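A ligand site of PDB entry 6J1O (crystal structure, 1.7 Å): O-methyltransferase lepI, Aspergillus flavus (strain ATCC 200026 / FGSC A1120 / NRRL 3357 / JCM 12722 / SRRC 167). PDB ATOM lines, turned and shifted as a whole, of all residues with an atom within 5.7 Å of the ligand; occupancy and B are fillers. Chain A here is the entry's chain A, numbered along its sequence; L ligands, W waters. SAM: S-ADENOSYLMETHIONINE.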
ATOM      1  N   LEU A 193      12.097  -8.338 -11.710  1.00  0.00           N
ATOM      2  CA  LEU A 193      12.984  -9.438 -12.090  1.00  0.00           C
ATOM      3  C   LEU A 193      13.789  -9.152 -13.358  1.00  0.00           C
ATOM      4  O   LEU A 193      14.778  -9.840 -13.615  1.00  0.00           O
ATOM      5  CB  LEU A 193      12.184 -10.725 -12.284  1.00  0.00           C
ATOM      6  CG  LEU A 193      11.676 -11.395 -11.006  1.00  0.00           C
ATOM      7  CD1 LEU A 193      10.885 -12.637 -11.365  1.00  0.00           C
ATOM      8  CD2 LEU A 193      12.837 -11.756 -10.089  1.00  0.00           C
ATOM      9  N   ASP A 225      20.268 -23.385 -12.390  1.00  0.00           N
ATOM     10  CA  ASP A 225      20.015 -22.064 -11.805  1.00  0.00           C
ATOM     11  C   ASP A 225      18.706 -22.136 -11.044  1.00  0.00           C
ATOM     12  O   ASP A 225      17.629 -21.994 -11.628  1.00  0.00           O
ATOM     13  CB  ASP A 225      19.973 -21.035 -12.937  1.00  0.00           C
ATOM     14  CG  ASP A 225      19.988 -19.600 -12.449  1.00  0.00           C
ATOM     15  OD1 ASP A 225      20.067 -19.343 -11.234  1.00  0.00           O
ATOM     16  OD2 ASP A 225      19.920 -18.715 -13.341  1.00  0.00           O
ATOM     17  N   ILE A 226      18.795 -22.347  -9.725  1.00  0.00           N
ATOM     18  CA  ILE A 226      17.631 -22.681  -8.906  1.00  0.00           C
ATOM     19  C   ILE A 226      16.974 -21.389  -8.419  1.00  0.00           C
ATOM     20  O   ILE A 226      17.585 -20.619  -7.673  1.00  0.00           O
ATOM     21  CB  ILE A 226      18.028 -23.579  -7.728  1.00  0.00           C
ATOM     22  CG1 ILE A 226      18.707 -24.862  -8.234  1.00  0.00           C
ATOM     23  CG2 ILE A 226      16.810 -23.910  -6.890  1.00  0.00           C
ATOM     24  CD1 ILE A 226      19.329 -25.696  -7.134  1.00  0.00           C
ATOM     25  N   GLY A 227      15.734 -21.156  -8.838  1.00  0.00           N
ATOM     26  CA  GLY A 227      15.120 -19.857  -8.642  1.00  0.00           C
ATOM     27  C   GLY A 227      15.791 -18.782  -9.471  1.00  0.00           C
ATOM     28  O   GLY A 227      16.011 -17.663  -8.989  1.00  0.00           O
ATOM     29  N   GLY A 228      16.134 -19.092 -10.725  1.00  0.00           N
ATOM     30  CA  GLY A 228      16.929 -18.201 -11.542  1.00  0.00           C
ATOM     31  C   GLY A 228      16.201 -17.011 -12.137  1.00  0.00           C
ATOM     32  O   GLY A 228      16.840 -16.180 -12.801  1.00  0.00           O
ATOM     33  N   GLY A 229      14.896 -16.887 -11.932  1.00  0.00           N
ATOM     34  CA  GLY A 229      14.199 -15.698 -12.418  1.00  0.00           C
ATOM     35  C   GLY A 229      14.192 -15.648 -13.931  1.00  0.00           C
ATOM     36  O   GLY A 229      13.762 -16.595 -14.596  1.00  0.00           O
ATOM     37  N   MET A 230      14.671 -14.534 -14.491  1.00  0.00           N
ATOM     38  CA  MET A 230      14.767 -14.401 -15.943  1.00  0.00           C
ATOM     39  C   MET A 230      15.918 -15.212 -16.527  1.00  0.00           C
ATOM     40  O   MET A 230      16.030 -15.296 -17.762  1.00  0.00           O
ATOM     41  CB  MET A 230      14.931 -12.925 -16.316  1.00  0.00           C
ATOM     42  CG  MET A 230      13.737 -12.060 -15.919  1.00  0.00           C
ATOM     43  SD  MET A 230      12.201 -12.533 -16.734  1.00  0.00           S
ATOM     44  CE  MET A 230      11.395 -13.516 -15.466  1.00  0.00           C
ATOM     45  N   HIS A 232      19.289 -14.666 -16.030  1.00  0.00           N
ATOM     46  CA  HIS A 232      20.460 -13.850 -16.367  1.00  0.00           C
ATOM     47  C   HIS A 232      21.755 -14.604 -16.124  1.00  0.00           C
ATOM     48  O   HIS A 232      22.698 -14.490 -16.912  1.00  0.00           O
ATOM     49  CB  HIS A 232      20.454 -12.548 -15.565  1.00  0.00           C
ATOM     50  CG  HIS A 232      19.281 -11.662 -15.831  1.00  0.00           C
ATOM     51  ND1 HIS A 232      18.598 -11.012 -14.819  1.00  0.00           N
ATOM     52  CD2 HIS A 232      18.671 -11.317 -16.982  1.00  0.00           C
ATOM     53  CE1 HIS A 232      17.615 -10.306 -15.348  1.00  0.00           C
ATOM     54  NE2 HIS A 232      17.632 -10.465 -16.658  1.00  0.00           N
ATOM     55  N   ALA A 233      21.832 -15.384 -15.043  1.00  0.00           N
ATOM     56  CA  ALA A 233      23.059 -16.122 -14.758  1.00  0.00           C
ATOM     57  C   ALA A 233      23.336 -17.144 -15.844  1.00  0.00           C
ATOM     58  O   ALA A 233      24.487 -17.314 -16.266  1.00  0.00           O
ATOM     59  CB  ALA A 233      22.980 -16.814 -13.390  1.00  0.00           C
ATOM     60  N   GLN A 251      15.661 -23.019 -13.553  1.00  0.00           N
ATOM     61  CA  GLN A 251      14.569 -23.561 -12.750  1.00  0.00           C
ATOM     62  C   GLN A 251      13.865 -22.421 -12.017  1.00  0.00           C
ATOM     63  O   GLN A 251      14.521 -21.629 -11.338  1.00  0.00           O
ATOM     64  CB  GLN A 251      15.087 -24.580 -11.729  1.00  0.00           C
ATOM     65  CG  GLN A 251      15.472 -25.925 -12.354  1.00  0.00           C
ATOM     66  CD  GLN A 251      16.011 -26.903 -11.332  1.00  0.00           C
ATOM     67  OE1 GLN A 251      16.329 -26.528 -10.207  1.00  0.00           O
ATOM     68  NE2 GLN A 251      16.111 -28.173 -11.722  1.00  0.00           N
ATOM     69  N   ASP A 252      12.544 -22.368 -12.155  1.00  0.00           N
ATOM     70  CA  ASP A 252      11.725 -21.376 -11.438  1.00  0.00           C
ATOM     71  C   ASP A 252      10.272 -21.841 -11.523  1.00  0.00           C
ATOM     72  O   ASP A 252       9.983 -22.930 -12.011  1.00  0.00           O
ATOM     73  CB  ASP A 252      11.938 -19.979 -12.008  1.00  0.00           C
ATOM     74  CG  ASP A 252      11.778 -18.889 -10.948  1.00  0.00           C
ATOM     75  OD1 ASP A 252      10.659 -18.702 -10.414  1.00  0.00           O
ATOM     76  OD2 ASP A 252      12.790 -18.206 -10.648  1.00  0.00           O
ATOM     77  N   LEU A 253       9.356 -21.010 -11.038  1.00  0.00           N
ATOM     78  CA  LEU A 253       7.949 -21.363 -11.125  1.00  0.00           C
ATOM     79  C   LEU A 253       7.396 -21.010 -12.508  1.00  0.00           C
ATOM     80  O   LEU A 253       7.922 -20.118 -13.181  1.00  0.00           O
ATOM     81  CB  LEU A 253       7.169 -20.664 -10.016  1.00  0.00           C
ATOM     82  CG  LEU A 253       7.693 -21.012  -8.626  1.00  0.00           C
ATOM     83  CD1 LEU A 253       6.961 -20.214  -7.549  1.00  0.00           C
ATOM     84  CD2 LEU A 253       7.592 -22.519  -8.355  1.00  0.00           C
ATOM     85  N   VAL A 256       7.013 -17.256 -13.906  1.00  0.00           N
ATOM     86  CA  VAL A 256       8.222 -16.487 -14.206  1.00  0.00           C
ATOM     87  C   VAL A 256       9.010 -17.132 -15.355  1.00  0.00           C
ATOM     88  O   VAL A 256       9.626 -16.414 -16.146  1.00  0.00           O
ATOM     89  CB  VAL A 256       9.051 -16.214 -12.935  1.00  0.00           C
ATOM     90  CG1 VAL A 256       8.440 -16.896 -11.722  1.00  0.00           C
ATOM     91  CG2 VAL A 256      10.523 -16.521 -13.105  1.00  0.00           C
ATOM     92  N   HIS A 274      10.247 -25.923 -11.499  1.00  0.00           N
ATOM     93  CA  HIS A 274      10.700 -26.636 -10.309  1.00  0.00           C
ATOM     94  C   HIS A 274      10.489 -25.757  -9.099  1.00  0.00           C
ATOM     95  O   HIS A 274      10.935 -24.611  -9.074  1.00  0.00           O
ATOM     96  CB  HIS A 274      12.179 -27.024 -10.412  1.00  0.00           C
ATOM     97  CG  HIS A 274      12.740 -27.592  -9.143  1.00  0.00           C
ATOM     98  ND1 HIS A 274      12.156 -28.660  -8.501  1.00  0.00           N
ATOM     99  CD2 HIS A 274      13.825 -27.245  -8.406  1.00  0.00           C
ATOM    100  CE1 HIS A 274      12.859 -28.949  -7.408  1.00  0.00           C
ATOM    101  NE2 HIS A 274      13.867 -28.101  -7.325  1.00  0.00           N
ATOM    102  N   ASN A 275       9.819 -26.306  -8.089  1.00  0.00           N
ATOM    103  CA  ASN A 275       9.651 -25.649  -6.813  1.00  0.00           C
ATOM    104  C   ASN A 275      10.825 -26.059  -5.924  1.00  0.00           C
ATOM    105  O   ASN A 275      11.010 -27.266  -5.668  1.00  0.00           O
ATOM    106  CB  ASN A 275       8.309 -26.031  -6.198  1.00  0.00           C
ATOM    107  CG  ASN A 275       7.999 -25.272  -4.934  1.00  0.00           C
ATOM    108  OD1 ASN A 275       8.869 -25.063  -4.095  1.00  0.00           O
ATOM    109  ND2 ASN A 275       6.751 -24.839  -4.789  1.00  0.00           N
ATOM    110  N   PHE A 276      11.633 -25.096  -5.467  1.00  0.00           N
ATOM    111  CA  PHE A 276      12.844 -25.483  -4.752  1.00  0.00           C
ATOM    112  C   PHE A 276      12.572 -25.945  -3.320  1.00  0.00           C
ATOM    113  O   PHE A 276      13.527 -26.262  -2.599  1.00  0.00           O
ATOM    114  CB  PHE A 276      13.911 -24.369  -4.794  1.00  0.00           C
ATOM    115  CG  PHE A 276      13.473 -22.981  -4.330  1.00  0.00           C
ATOM    116  CD1 PHE A 276      12.835 -22.786  -3.111  1.00  0.00           C
ATOM    117  CD2 PHE A 276      13.809 -21.865  -5.077  1.00  0.00           C
ATOM    118  CE1 PHE A 276      12.480 -21.508  -2.690  1.00  0.00           C
ATOM    119  CE2 PHE A 276      13.462 -20.579  -4.668  1.00  0.00           C
ATOM    120  CZ  PHE A 276      12.793 -20.404  -3.468  1.00  0.00           C
ATOM    121  N   HIS A 277      11.312 -26.026  -2.902  1.00  0.00           N
ATOM    122  CA  HIS A 277      10.941 -26.723  -1.672  1.00  0.00           C
ATOM    123  C   HIS A 277      10.700 -28.213  -1.893  1.00  0.00           C
ATOM    124  O   HIS A 277      10.206 -28.887  -0.982  1.00  0.00           O
ATOM    125  CB  HIS A 277       9.701 -26.078  -1.041  1.00  0.00           C
ATOM    126  CG  HIS A 277       9.911 -24.664  -0.611  1.00  0.00           C
ATOM    127  ND1 HIS A 277      10.791 -24.310   0.381  1.00  0.00           N
ATOM    128  CD2 HIS A 277       9.350 -23.506  -1.052  1.00  0.00           C
ATOM    129  CE1 HIS A 277      10.771 -22.997   0.545  1.00  0.00           C
ATOM    130  NE2 HIS A 277       9.916 -22.487  -0.325  1.00  0.00           N
ATOM    131  N   LEU A 290      22.428 -20.896  -6.454  1.00  0.00           N
ATOM    132  CA  LEU A 290      21.390 -20.202  -5.697  1.00  0.00           C
ATOM    133  C   LEU A 290      21.815 -18.748  -5.480  1.00  0.00           C
ATOM    134  O   LEU A 290      22.580 -18.456  -4.568  1.00  0.00           O
ATOM    135  CB  LEU A 290      21.168 -20.880  -4.342  1.00  0.00           C
ATOM    136  CG  LEU A 290      20.564 -22.275  -4.307  1.00  0.00           C
ATOM    137  CD1 LEU A 290      20.930 -22.977  -3.005  1.00  0.00           C
ATOM    138  CD2 LEU A 290      19.057 -22.210  -4.481  1.00  0.00           C
ATOM    139  N   ARG A 291      21.306 -17.827  -6.294  1.00  0.00           N
ATOM    140  CA  ARG A 291      21.683 -16.418  -6.195  1.00  0.00           C
ATOM    141  C   ARG A 291      20.547 -15.620  -5.569  1.00  0.00           C
ATOM    142  O   ARG A 291      19.443 -15.570  -6.126  1.00  0.00           O
ATOM    143  CB  ARG A 291      22.043 -15.815  -7.555  1.00  0.00           C
ATOM    144  CG  ARG A 291      22.473 -14.345  -7.436  1.00  0.00           C
ATOM    145  CD  ARG A 291      23.246 -13.895  -8.664  1.00  0.00           C
ATOM    146  NE  ARG A 291      22.363 -13.793  -9.826  1.00  0.00           N
ATOM    147  CZ  ARG A 291      22.801 -13.689 -11.078  1.00  0.00           C
ATOM    148  NH1 ARG A 291      24.101 -13.690 -11.321  1.00  0.00           N
ATOM    149  NH2 ARG A 291      21.931 -13.591 -12.075  1.00  0.00           N
ATOM    150  N   LEU A 292      20.826 -14.997  -4.419  1.00  0.00           N
ATOM    151  CA  LEU A 292      19.854 -14.174  -3.702  1.00  0.00           C
ATOM    152  C   LEU A 292      18.570 -14.942  -3.405  1.00  0.00           C
ATOM    153  O   LEU A 292      17.461 -14.394  -3.472  1.00  0.00           O
ATOM    154  CB  LEU A 292      19.564 -12.871  -4.464  1.00  0.00           C
ATOM    155  CG  LEU A 292      20.757 -11.914  -4.627  1.00  0.00           C
ATOM    156  CD1 LEU A 292      20.354 -10.702  -5.438  1.00  0.00           C
ATOM    157  CD2 LEU A 292      21.335 -11.489  -3.279  1.00  0.00           C
ATOM    158  N   ILE A 293      18.725 -16.217  -3.061  1.00  0.00           N
ATOM    159  CA  ILE A 293      17.598 -17.066  -2.705  1.00  0.00           C
ATOM    160  C   ILE A 293      17.538 -17.250  -1.189  1.00  0.00           C
ATOM    161  O   ILE A 293      16.518 -16.929  -0.549  1.00  0.00           O
ATOM    162  CB  ILE A 293      17.684 -18.437  -3.407  1.00  0.00           C
ATOM    163  CG1 ILE A 293      17.682 -18.270  -4.922  1.00  0.00           C
ATOM    164  CG2 ILE A 293      16.546 -19.334  -2.937  1.00  0.00           C
ATOM    165  CD1 ILE A 293      16.495 -17.498  -5.451  1.00  0.00           C
ATOM    166  N   ASP A 296      16.344 -14.874   1.796  1.00  0.00           N
ATOM    167  CA  ASP A 296      14.949 -14.543   1.994  1.00  0.00           C
ATOM    168  C   ASP A 296      14.238 -15.528   2.916  1.00  0.00           C
ATOM    169  O   ASP A 296      13.024 -15.408   3.111  1.00  0.00           O
ATOM    170  CB  ASP A 296      14.227 -14.470   0.643  1.00  0.00           C
ATOM    171  CG  ASP A 296      14.541 -13.178  -0.105  1.00  0.00           C
ATOM    172  OD1 ASP A 296      15.120 -12.257   0.506  1.00  0.00           O
ATOM    173  OD2 ASP A 296      14.204 -13.079  -1.304  1.00  0.00           O
ATOM    174  N   PHE A 297      14.973 -16.461   3.517  1.00  0.00           N
ATOM    175  CA  PHE A 297      14.403 -17.496   4.381  1.00  0.00           C
ATOM    176  C   PHE A 297      15.143 -17.571   5.704  1.00  0.00           C
ATOM    177  O   PHE A 297      16.377 -17.471   5.740  1.00  0.00           O
ATOM    178  CB  PHE A 297      14.465 -18.867   3.678  1.00  0.00           C
ATOM    179  CG  PHE A 297      13.667 -18.937   2.420  1.00  0.00           C
ATOM    180  CD1 PHE A 297      12.328 -19.259   2.458  1.00  0.00           C
ATOM    181  CD2 PHE A 297      14.253 -18.627   1.195  1.00  0.00           C
ATOM    182  CE1 PHE A 297      11.579 -19.297   1.287  1.00  0.00           C
ATOM    183  CE2 PHE A 297      13.508 -18.655   0.034  1.00  0.00           C
ATOM    184  CZ  PHE A 297      12.169 -18.996   0.082  1.00  0.00           C
HETATM  185  N   SAM L   1      18.310 -16.020  -8.761  1.00  0.00           N
HETATM  186  CA  SAM L   1      17.664 -14.792  -9.202  1.00  0.00           C
HETATM  187  C   SAM L   1      18.692 -13.808  -9.735  1.00  0.00           C
HETATM  188  O   SAM L   1      18.615 -13.350 -10.883  1.00  0.00           O
HETATM  189  OXT SAM L   1      19.653 -13.445  -9.052  1.00  0.00           O
HETATM  190  CB  SAM L   1      16.872 -14.178  -8.036  1.00  0.00           C
HETATM  191  CG  SAM L   1      15.465 -13.796  -8.432  1.00  0.00           C
HETATM  192  SD  SAM L   1      14.381 -13.399  -7.044  1.00  0.00           S
HETATM  193  CE  SAM L   1      15.503 -12.792  -5.754  1.00  0.00           C
HETATM  194  C5' SAM L   1      13.891 -15.004  -6.379  1.00  0.00           C
HETATM  195  C4' SAM L   1      13.406 -15.992  -7.441  1.00  0.00           C
HETATM  196  O4' SAM L   1      12.966 -17.154  -6.764  1.00  0.00           O
HETATM  197  C3' SAM L   1      12.226 -15.482  -8.263  1.00  0.00           C
HETATM  198  O3' SAM L   1      12.508 -15.637  -9.645  1.00  0.00           O
HETATM  199  C2' SAM L   1      11.066 -16.357  -7.820  1.00  0.00           C
HETATM  200  O2' SAM L   1      10.101 -16.640  -8.812  1.00  0.00           O
HETATM  201  C1' SAM L   1      11.798 -17.617  -7.402  1.00  0.00           C
HETATM  202  N9  SAM L   1      11.031 -18.451  -6.472  1.00  0.00           N
HETATM  203  C8  SAM L   1      10.272 -18.045  -5.397  1.00  0.00           C
HETATM  204  N7  SAM L   1       9.748 -19.150  -4.816  1.00  0.00           N
HETATM  205  C5  SAM L   1      10.177 -20.236  -5.517  1.00  0.00           C
HETATM  206  C6  SAM L   1       9.952 -21.605  -5.373  1.00  0.00           C
HETATM  207  N6  SAM L   1       9.199 -22.061  -4.389  1.00  0.00           N
HETATM  208  N1  SAM L   1      10.540 -22.485  -6.263  1.00  0.00           N
HETATM  209  C2  SAM L   1      11.327 -22.016  -7.287  1.00  0.00           C
HETATM  210  N3  SAM L   1      11.540 -20.664  -7.441  1.00  0.00           N
HETATM  211  C4  SAM L   1      10.968 -19.806  -6.555  1.00  0.00           C
HETATM  212  O   HOH W   1      14.687 -14.938  -3.070  1.00  0.00           O
HETATM  213  O   HOH W   2      16.293 -11.994  -2.692  1.00  0.00           O
HETATM  214  O   HOH W   3      17.893 -13.647 -13.609  1.00  0.00           O
HETATM  215  O   HOH W   4      19.455 -18.781  -8.482  1.00  0.00           O
HETATM  216  O   HOH W   5       7.157 -21.187  -2.497  1.00  0.00           O
HETATM  217  O   HOH W   6      20.340 -16.607 -10.663  1.00  0.00           O
HETATM  218  O   HOH W   7       7.442 -16.673  -8.106  1.00  0.00           O
HETATM  219  O   HOH W   8      20.701 -10.952  -8.697  1.00  0.00           O
HETATM  220  O   HOH W   9       9.282 -18.161  -2.209  1.00  0.00           O
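OD1 of Asn 275 sits at hydrogen-bond distance from N6 of the ligand, at 3.0 Å. OD1 of Asp 252 lies within hydrogen-bond range of O2' of the ligand, 2.7 Å away. The backbone NH (N) of Phe 276 sits at hydrogen-bond distance from a nitrogen (N1) of the ligand (2.9 Å). O of Arg 291 sits at hydrogen-bond distance from N of the ligand, 2.9 Å away. A nitrogen (N) of the ligand is in hydrogen-bond range of the backbone carbonyl oxygen of Gly 227 (2.8 Å). OXT of the ligand lies within salt-bridge range of NE of Arg 291 (2.8 Å).
The backbone NH of Gly 228 sits at hydrogen-bond distance from the side-chain carboxylate of Asp 252, at 3.5 Å. O of Gln 251 is in hydrogen-bond range of N of Gly 227 (2.8 Å). The backbone carbonyl oxygen (O) of Asp 252 is in hydrogen-bond range of the backbone NH (N) of His 274, at 3.0 Å. The backbone NH (N) of Gly 228 is in hydrogen-bond range of the backbone carbonyl oxygen (O) of Gln 251, at 3.1 Å. OD1 of Asn 275 is in hydrogen-bond range of N of His 277, 2.9 Å away. The side-chain carboxylate of Asp 252 is in hydrogen-bond range of the backbone NH of Gly 229, 2.8 Å away.
Leu 193 touches the ligand (CD2 to CG, 3.7 Å). Gly 228 touches the ligand (CA to N, 3.8 Å). CA of Gly 229 touches O3' of the ligand, 3.2 Å away. CD2 of Leu 253 touches N1 of the ligand (3.6 Å). Val 256 touches the ligand (CG1 to O2', 3.4 Å). His 274 touches the ligand (O to C2, 3.2 Å). CD2 of His 277 touches N6 of the ligand, at 3.6 Å. Leu 292 touches the ligand (O to CE, 3.4 Å). Ile 293 touches the ligand (CD1 to C5', 3.7 Å). Hydrophobic or aromatic side chains that line the ligand: Leu 193, Leu 253, Val 256, Phe 276, His 277 and Ile 293. Of the 23 residues printed, 14 come within 4 Å of the ligand. The nearest printed residue that does not touch the ligand is Asp 225 (4.5 Å).
Water W8 bridges an oxygen (OXT) of the ligand (2.7 Å) and the guanidinium group of Arg 291 (3.5 Å). Water W3 lies within hydrogen-bond range of an oxygen (O) of the ligand, the backbone carbonyl oxygen (O) of Gly 228, the backbone NH (N) of His 232 and the backbone NH (N) of Met 230. Water W6 bridges OD1 of Asp 225 (2.8 Å) and N of the ligand (2.8 Å). Water W4 lies within hydrogen-bond range of O of Ile 226 (2.7 Å), OD1 of Asp 225 (2.9 Å), N of the ligand (3.0 Å) and N of Arg 291 (3.0 Å). Water W2 lies within hydrogen-bond range of the side-chain carboxylate of Asp 296 (2.7 Å) and the backbone carbonyl oxygen of Leu 292 (2.8 Å). Water W1 lies within hydrogen-bond range of OD2 of Asp 296 (2.6 Å) and O of Leu 292 (2.9 Å).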
